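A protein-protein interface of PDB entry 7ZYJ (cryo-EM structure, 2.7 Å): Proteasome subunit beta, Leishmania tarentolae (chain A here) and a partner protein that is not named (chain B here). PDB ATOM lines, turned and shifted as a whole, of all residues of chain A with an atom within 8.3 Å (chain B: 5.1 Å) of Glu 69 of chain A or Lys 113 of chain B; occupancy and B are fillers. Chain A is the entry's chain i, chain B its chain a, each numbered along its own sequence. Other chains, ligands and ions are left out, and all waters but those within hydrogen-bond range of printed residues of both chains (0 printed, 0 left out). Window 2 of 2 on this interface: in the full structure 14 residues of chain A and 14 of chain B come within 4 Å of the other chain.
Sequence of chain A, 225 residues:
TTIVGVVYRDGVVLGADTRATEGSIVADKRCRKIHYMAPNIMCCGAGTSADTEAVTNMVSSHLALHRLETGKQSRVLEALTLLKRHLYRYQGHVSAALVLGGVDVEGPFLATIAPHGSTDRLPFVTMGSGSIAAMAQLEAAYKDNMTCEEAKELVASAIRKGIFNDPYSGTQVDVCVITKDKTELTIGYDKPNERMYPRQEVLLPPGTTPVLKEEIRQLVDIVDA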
ATOM      1  N   HIS A  62       1.659 -30.017  15.192  1.00  0.00           N
ATOM      2  CA  HIS A  62       2.816 -29.168  15.443  1.00  0.00           C
ATOM      3  C   HIS A  62       3.677 -29.736  16.565  1.00  0.00           C
ATOM      4  O   HIS A  62       4.910 -29.701  16.490  1.00  0.00           O
ATOM      5  CB  HIS A  62       2.357 -27.749  15.773  1.00  0.00           C
ATOM      6  CG  HIS A  62       3.476 -26.762  15.891  1.00  0.00           C
ATOM      7  ND1 HIS A  62       3.903 -25.989  14.833  1.00  0.00           N
ATOM      8  CD2 HIS A  62       4.264 -26.430  16.941  1.00  0.00           C
ATOM      9  CE1 HIS A  62       4.901 -25.219  15.228  1.00  0.00           C
ATOM     10  NE2 HIS A  62       5.140 -25.468  16.503  1.00  0.00           N
ATOM     11  N   LEU A  63       3.044 -30.272  17.611  1.00  0.00           N
ATOM     12  CA  LEU A  63       3.794 -30.904  18.691  1.00  0.00           C
ATOM     13  C   LEU A  63       4.542 -32.135  18.204  1.00  0.00           C
ATOM     14  O   LEU A  63       5.677 -32.378  18.617  1.00  0.00           O
ATOM     15  CB  LEU A  63       2.860 -31.277  19.841  1.00  0.00           C
ATOM     16  CG  LEU A  63       2.361 -30.163  20.757  1.00  0.00           C
ATOM     17  CD1 LEU A  63       1.610 -30.771  21.923  1.00  0.00           C
ATOM     18  CD2 LEU A  63       3.512 -29.301  21.247  1.00  0.00           C
ATOM     19  N   ALA A  64       3.912 -32.942  17.347  1.00  0.00           N
ATOM     20  CA  ALA A  64       4.599 -34.111  16.806  1.00  0.00           C
ATOM     21  C   ALA A  64       5.825 -33.699  16.003  1.00  0.00           C
ATOM     22  O   ALA A  64       6.902 -34.298  16.135  1.00  0.00           O
ATOM     23  CB  ALA A  64       3.642 -34.935  15.947  1.00  0.00           C
ATOM     24  N   LEU A  65       5.684 -32.660  15.178  1.00  0.00           N
ATOM     25  CA  LEU A  65       6.832 -32.135  14.443  1.00  0.00           C
ATOM     26  C   LEU A  65       7.911 -31.642  15.401  1.00  0.00           C
ATOM     27  O   LEU A  65       9.110 -31.861  15.179  1.00  0.00           O
ATOM     28  CB  LEU A  65       6.382 -31.010  13.511  1.00  0.00           C
ATOM     29  CG  LEU A  65       7.275 -30.723  12.305  1.00  0.00           C
ATOM     30  CD1 LEU A  65       7.128 -31.821  11.270  1.00  0.00           C
ATOM     31  CD2 LEU A  65       6.946 -29.369  11.702  1.00  0.00           C
ATOM     32  N   HIS A  66       7.499 -30.971  16.478  1.00  0.00           N
ATOM     33  CA  HIS A  66       8.461 -30.449  17.440  1.00  0.00           C
ATOM     34  C   HIS A  66       9.213 -31.564  18.157  1.00  0.00           C
ATOM     35  O   HIS A  66      10.413 -31.437  18.401  1.00  0.00           O
ATOM     36  CB  HIS A  66       7.754 -29.546  18.447  1.00  0.00           C
ATOM     37  CG  HIS A  66       8.685 -28.856  19.391  1.00  0.00           C
ATOM     38  ND1 HIS A  66       8.729 -29.146  20.738  1.00  0.00           N
ATOM     39  CD2 HIS A  66       9.607 -27.888  19.183  1.00  0.00           C
ATOM     40  CE1 HIS A  66       9.642 -28.387  21.318  1.00  0.00           C
ATOM     41  NE2 HIS A  66      10.188 -27.614  20.397  1.00  0.00           N
ATOM     42  N   ARG A  67       8.532 -32.659  18.506  1.00  0.00           N
ATOM     43  CA  ARG A  67       9.234 -33.778  19.131  1.00  0.00           C
ATOM     44  C   ARG A  67      10.117 -34.515  18.137  1.00  0.00           C
ATOM     45  O   ARG A  67      11.125 -35.108  18.534  1.00  0.00           O
ATOM     46  CB  ARG A  67       8.257 -34.766  19.771  1.00  0.00           C
ATOM     47  CG  ARG A  67       7.103 -34.149  20.515  1.00  0.00           C
ATOM     48  CD  ARG A  67       6.395 -35.190  21.356  1.00  0.00           C
ATOM     49  NE  ARG A  67       6.027 -36.353  20.558  1.00  0.00           N
ATOM     50  CZ  ARG A  67       4.815 -36.564  20.063  1.00  0.00           C
ATOM     51  NH1 ARG A  67       3.827 -35.712  20.267  1.00  0.00           N
ATOM     52  NH2 ARG A  67       4.593 -37.658  19.340  1.00  0.00           N
ATOM     53  N   LEU A  68       9.759 -34.503  16.854  1.00  0.00           N
ATOM     54  CA  LEU A  68      10.685 -35.014  15.851  1.00  0.00           C
ATOM     55  C   LEU A  68      11.943 -34.157  15.791  1.00  0.00           C
ATOM     56  O   LEU A  68      13.055 -34.679  15.649  1.00  0.00           O
ATOM     57  CB  LEU A  68      10.009 -35.072  14.483  1.00  0.00           C
ATOM     58  CG  LEU A  68       9.240 -36.356  14.174  1.00  0.00           C
ATOM     59  CD1 LEU A  68       8.707 -36.325  12.754  1.00  0.00           C
ATOM     60  CD2 LEU A  68      10.123 -37.572  14.393  1.00  0.00           C
ATOM     61  N   GLU A  69      11.783 -32.837  15.901  1.00  0.00           N
ATOM     62  CA  GLU A  69      12.932 -31.937  15.862  1.00  0.00           C
ATOM     63  C   GLU A  69      13.814 -32.098  17.098  1.00  0.00           C
ATOM     64  O   GLU A  69      15.037 -32.247  16.988  1.00  0.00           O
ATOM     65  CB  GLU A  69      12.453 -30.490  15.729  1.00  0.00           C
ATOM     66  CG  GLU A  69      13.563 -29.459  15.816  1.00  0.00           C
ATOM     67  CD  GLU A  69      13.058 -28.043  15.629  1.00  0.00           C
ATOM     68  OE1 GLU A  69      12.550 -27.459  16.610  1.00  0.00           O
ATOM     69  OE2 GLU A  69      13.167 -27.514  14.504  1.00  0.00           O
ATOM     70  N   THR A  70      13.212 -32.072  18.290  1.00  0.00           N
ATOM     71  CA  THR A  70      13.994 -32.054  19.523  1.00  0.00           C
ATOM     72  C   THR A  70      14.406 -33.453  19.965  1.00  0.00           C
ATOM     73  O   THR A  70      15.512 -33.638  20.485  1.00  0.00           O
ATOM     74  CB  THR A  70      13.208 -31.373  20.646  1.00  0.00           C
ATOM     75  OG1 THR A  70      12.192 -32.259  21.131  1.00  0.00           O
ATOM     76  CG2 THR A  70      12.559 -30.091  20.154  1.00  0.00           C
ATOM     77  N   GLY A  71      13.540 -34.445  19.772  1.00  0.00           N
ATOM     78  CA  GLY A  71      13.788 -35.780  20.265  1.00  0.00           C
ATOM     79  C   GLY A  71      13.326 -36.032  21.683  1.00  0.00           C
ATOM     80  O   GLY A  71      13.444 -37.167  22.164  1.00  0.00           O
ATOM     81  N   LYS A  72      12.808 -35.018  22.366  1.00  0.00           N
ATOM     82  CA  LYS A  72      12.278 -35.162  23.711  1.00  0.00           C
ATOM     83  C   LYS A  72      10.774 -35.413  23.659  1.00  0.00           C
ATOM     84  O   LYS A  72      10.146 -35.379  22.600  1.00  0.00           O
ATOM     85  CB  LYS A  72      12.571 -33.911  24.537  1.00  0.00           C
ATOM     86  CG  LYS A  72      14.040 -33.560  24.662  1.00  0.00           C
ATOM     87  CD  LYS A  72      14.782 -34.553  25.533  1.00  0.00           C
ATOM     88  CE  LYS A  72      16.253 -34.190  25.624  1.00  0.00           C
ATOM     89  NZ  LYS A  72      16.454 -32.906  26.350  1.00  0.00           N
ATOM     90  N   TYR B  98      11.517 -18.511  20.001  1.00  0.00           N
ATOM     91  CA  TYR B  98      11.180 -19.826  20.533  1.00  0.00           C
ATOM     92  C   TYR B  98      10.494 -19.690  21.883  1.00  0.00           C
ATOM     93  O   TYR B  98       9.423 -20.269  22.111  1.00  0.00           O
ATOM     94  CB  TYR B  98      12.445 -20.678  20.647  1.00  0.00           C
ATOM     95  CG  TYR B  98      12.197 -22.135  20.971  1.00  0.00           C
ATOM     96  CD1 TYR B  98      11.939 -22.544  22.272  1.00  0.00           C
ATOM     97  CD2 TYR B  98      12.238 -23.103  19.978  1.00  0.00           C
ATOM     98  CE1 TYR B  98      11.717 -23.868  22.572  1.00  0.00           C
ATOM     99  CE2 TYR B  98      12.019 -24.433  20.271  1.00  0.00           C
ATOM    100  CZ  TYR B  98      11.759 -24.809  21.570  1.00  0.00           C
ATOM    101  OH  TYR B  98      11.539 -26.131  21.870  1.00  0.00           O
ATOM    102  N   ILE B 108      19.421 -26.540  24.126  1.00  0.00           N
ATOM    103  CA  ILE B 108      20.695 -26.213  23.492  1.00  0.00           C
ATOM    104  C   ILE B 108      20.842 -26.940  22.160  1.00  0.00           C
ATOM    105  O   ILE B 108      21.325 -26.365  21.176  1.00  0.00           O
ATOM    106  CB  ILE B 108      21.865 -26.516  24.448  1.00  0.00           C
ATOM    107  CG1 ILE B 108      23.199 -26.151  23.792  1.00  0.00           C
ATOM    108  CG2 ILE B 108      21.844 -27.969  24.908  1.00  0.00           C
ATOM    109  CD1 ILE B 108      24.376 -26.224  24.728  1.00  0.00           C
ATOM    110  N   ALA B 109      20.430 -28.209  22.100  1.00  0.00           N
ATOM    111  CA  ALA B 109      20.541 -28.964  20.857  1.00  0.00           C
ATOM    112  C   ALA B 109      19.653 -28.374  19.769  1.00  0.00           C
ATOM    113  O   ALA B 109      20.057 -28.298  18.604  1.00  0.00           O
ATOM    114  CB  ALA B 109      20.192 -30.431  21.101  1.00  0.00           C
ATOM    115  N   VAL B 110      18.442 -27.950  20.131  1.00  0.00           N
ATOM    116  CA  VAL B 110      17.544 -27.330  19.163  1.00  0.00           C
ATOM    117  C   VAL B 110      18.130 -26.023  18.649  1.00  0.00           C
ATOM    118  O   VAL B 110      18.067 -25.726  17.449  1.00  0.00           O
ATOM    119  CB  VAL B 110      16.156 -27.121  19.794  1.00  0.00           C
ATOM    120  CG1 VAL B 110      15.191 -26.526  18.779  1.00  0.00           C
ATOM    121  CG2 VAL B 110      15.635 -28.429  20.341  1.00  0.00           C
ATOM    122  N   LEU B 111      18.696 -25.215  19.548  1.00  0.00           N
ATOM    123  CA  LEU B 111      19.317 -23.963  19.132  1.00  0.00           C
ATOM    124  C   LEU B 111      20.487 -24.216  18.194  1.00  0.00           C
ATOM    125  O   LEU B 111      20.651 -23.513  17.191  1.00  0.00           O
ATOM    126  CB  LEU B 111      19.771 -23.171  20.358  1.00  0.00           C
ATOM    127  CG  LEU B 111      20.589 -21.906  20.088  1.00  0.00           C
ATOM    128  CD1 LEU B 111      19.702 -20.797  19.551  1.00  0.00           C
ATOM    129  CD2 LEU B 111      21.309 -21.460  21.347  1.00  0.00           C
ATOM    130  N   ALA B 112      21.315 -25.216  18.504  1.00  0.00           N
ATOM    131  CA  ALA B 112      22.437 -25.544  17.630  1.00  0.00           C
ATOM    132  C   ALA B 112      21.954 -26.019  16.265  1.00  0.00           C
ATOM    133  O   ALA B 112      22.521 -25.644  15.233  1.00  0.00           O
ATOM    134  CB  ALA B 112      23.320 -26.602  18.288  1.00  0.00           C
ATOM    135  N   LYS B 113      20.904 -26.844  16.241  1.00  0.00           N
ATOM    136  CA  LYS B 113      20.357 -27.313  14.972  1.00  0.00           C
ATOM    137  C   LYS B 113      19.819 -26.155  14.141  1.00  0.00           C
ATOM    138  O   LYS B 113      20.032 -26.100  12.924  1.00  0.00           O
ATOM    139  CB  LYS B 113      19.262 -28.347  15.231  1.00  0.00           C
ATOM    140  CG  LYS B 113      18.604 -28.892  13.978  1.00  0.00           C
ATOM    141  CD  LYS B 113      17.139 -28.494  13.916  1.00  0.00           C
ATOM    142  CE  LYS B 113      16.544 -28.782  12.550  1.00  0.00           C
ATOM    143  NZ  LYS B 113      15.096 -28.445  12.492  1.00  0.00           N
ATOM    144  N   ARG B 114      19.129 -25.210  14.780  1.00  0.00           N
ATOM    145  CA  ARG B 114      18.593 -24.072  14.043  1.00  0.00           C
ATOM    146  C   ARG B 114      19.697 -23.136  13.560  1.00  0.00           C
ATOM    147  O   ARG B 114      19.597 -22.579  12.461  1.00  0.00           O
ATOM    148  CB  ARG B 114      17.580 -23.325  14.906  1.00  0.00           C
ATOM    149  CG  ARG B 114      16.192 -23.940  14.863  1.00  0.00           C
ATOM    150  CD  ARG B 114      15.364 -23.562  16.075  1.00  0.00           C
ATOM    151  NE  ARG B 114      14.104 -24.293  16.117  1.00  0.00           N
ATOM    152  CZ  ARG B 114      12.911 -23.722  16.210  1.00  0.00           C
ATOM    153  NH1 ARG B 114      12.778 -22.408  16.278  1.00  0.00           N
ATOM    154  NH2 ARG B 114      11.825 -24.488  16.238  1.00  0.00           N
ATOM    155  N   MET B 115      20.754 -22.957  14.356  1.00  0.00           N
ATOM    156  CA  MET B 115      21.890 -22.165  13.899  1.00  0.00           C
ATOM    157  C   MET B 115      22.603 -22.835  12.732  1.00  0.00           C
ATOM    158  O   MET B 115      23.077 -22.147  11.821  1.00  0.00           O
ATOM    159  CB  MET B 115      22.865 -21.922  15.050  1.00  0.00           C
ATOM    160  CG  MET B 115      22.317 -21.033  16.152  1.00  0.00           C
ATOM    161  SD  MET B 115      21.552 -19.529  15.522  1.00  0.00           S
ATOM    162  CE  MET B 115      22.981 -18.668  14.877  1.00  0.00           C
ATOM    163  N   GLY B 116      22.698 -24.165  12.745  1.00  0.00           N
ATOM    164  CA  GLY B 116      23.225 -24.871  11.592  1.00  0.00           C
ATOM    165  C   GLY B 116      22.340 -24.737  10.371  1.00  0.00           C
ATOM    166  O   GLY B 116      22.839 -24.669   9.244  1.00  0.00           O
ATOM    167  N   ASP B 117      21.022 -24.706  10.575  1.00  0.00           N
ATOM    168  CA  ASP B 117      20.107 -24.429   9.472  1.00  0.00           C
ATOM    169  C   ASP B 117      20.349 -23.043   8.891  1.00  0.00           C
ATOM    170  O   ASP B 117      20.321 -22.863   7.669  1.00  0.00           O
ATOM    171  CB  ASP B 117      18.658 -24.563   9.939  1.00  0.00           C
ATOM    172  CG  ASP B 117      18.227 -26.005  10.094  1.00  0.00           C
ATOM    173  OD1 ASP B 117      18.924 -26.897   9.570  1.00  0.00           O
ATOM    174  OD2 ASP B 117      17.185 -26.245  10.737  1.00  0.00           O
ATOM    175  N   THR B 162      26.281 -29.426  12.603  1.00  0.00           N
ATOM    176  CA  THR B 162      26.028 -29.303  14.030  1.00  0.00           C
ATOM    177  C   THR B 162      26.341 -30.622  14.720  1.00  0.00           C
ATOM    178  O   THR B 162      25.931 -31.689  14.258  1.00  0.00           O
ATOM    179  CB  THR B 162      24.573 -28.906  14.290  1.00  0.00           C
ATOM    180  OG1 THR B 162      24.361 -27.555  13.863  1.00  0.00           O
ATOM    181  CG2 THR B 162      24.234 -29.027  15.766  1.00  0.00           C
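Val 110 of chain B touches Glu 69 of chain A (CG1 to OE1, 3.5 Å). Val 110 of chain B touches Thr 70 of chain A (CG2 to CG2, 3.5 Å).
Of chain B, only Val 110 (3.5 Å), Lys 113 (2.9 Å) and Arg 114 (3.1 Å) come within 4 Å of Glu 69 of chain A. Of the printed residues of chain A, Lys 113 of chain B touches Glu 69. No residue of chain A comes within 4 Å of Ala 112 of chain B. Printed residues of chain B within 4 Å of Thr 70 of chain A: Val 110 (3.5 Å). Printed residues of chain A within 4 Å of Tyr 98 of chain B: His 66 (2.5 Å). Printed residues of chain A within 4 Å of Arg 114 of chain B: Glu 69. Ala 109 of chain B touches none of the printed residues of chain A. Gly 71 of chain A touches none of the printed residues of chain B. The nearest residue of chain B that does not touch Glu 69 of chain A is Tyr 98 of chain B (4.8 Å). The nearest residue of chain A that does not touch Lys 113 of chain B is Thr 70 of chain A (6.9 Å).
The side-chain amino group (NZ) of Lys 113 of chain B lies within salt-bridge range of the side-chain carboxylate (OD2) of Asp 117 of chain B, 3.5 Å away. OG1 of Thr 70 of chain A lies close to O of His 66 of chain A. The backbone NH of Lys 72 of chain A lies within hydrogen-bond range of the side-chain hydroxyl of Thr 70 of chain A, at 3.1 Å.
Printed residues of chain B that touch a printed residue of chain A: Tyr 98, Val 110, Lys 113 and Arg 114. Hydrophobic or aromatic side chains of chain B that line the printed part of chain A: Tyr 98 and Val 110. Hydrophobic or aromatic side chains of chain A within 4 Å of the printed part of chain B: His 66.
NE2 of His 66 of chain A is in hydrogen-bond range of OH of Tyr 98 of chain B (2.5 Å). NZ of Lys 113 of chain B is in salt-bridge range of OE2 of Glu 69 of chain A (2.9 Å). The guanidinium group (NH2) of Arg 114 of chain B lies within salt-bridge range of the side-chain carboxylate (OE1) of Glu 69 of chain A (3.1 Å).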
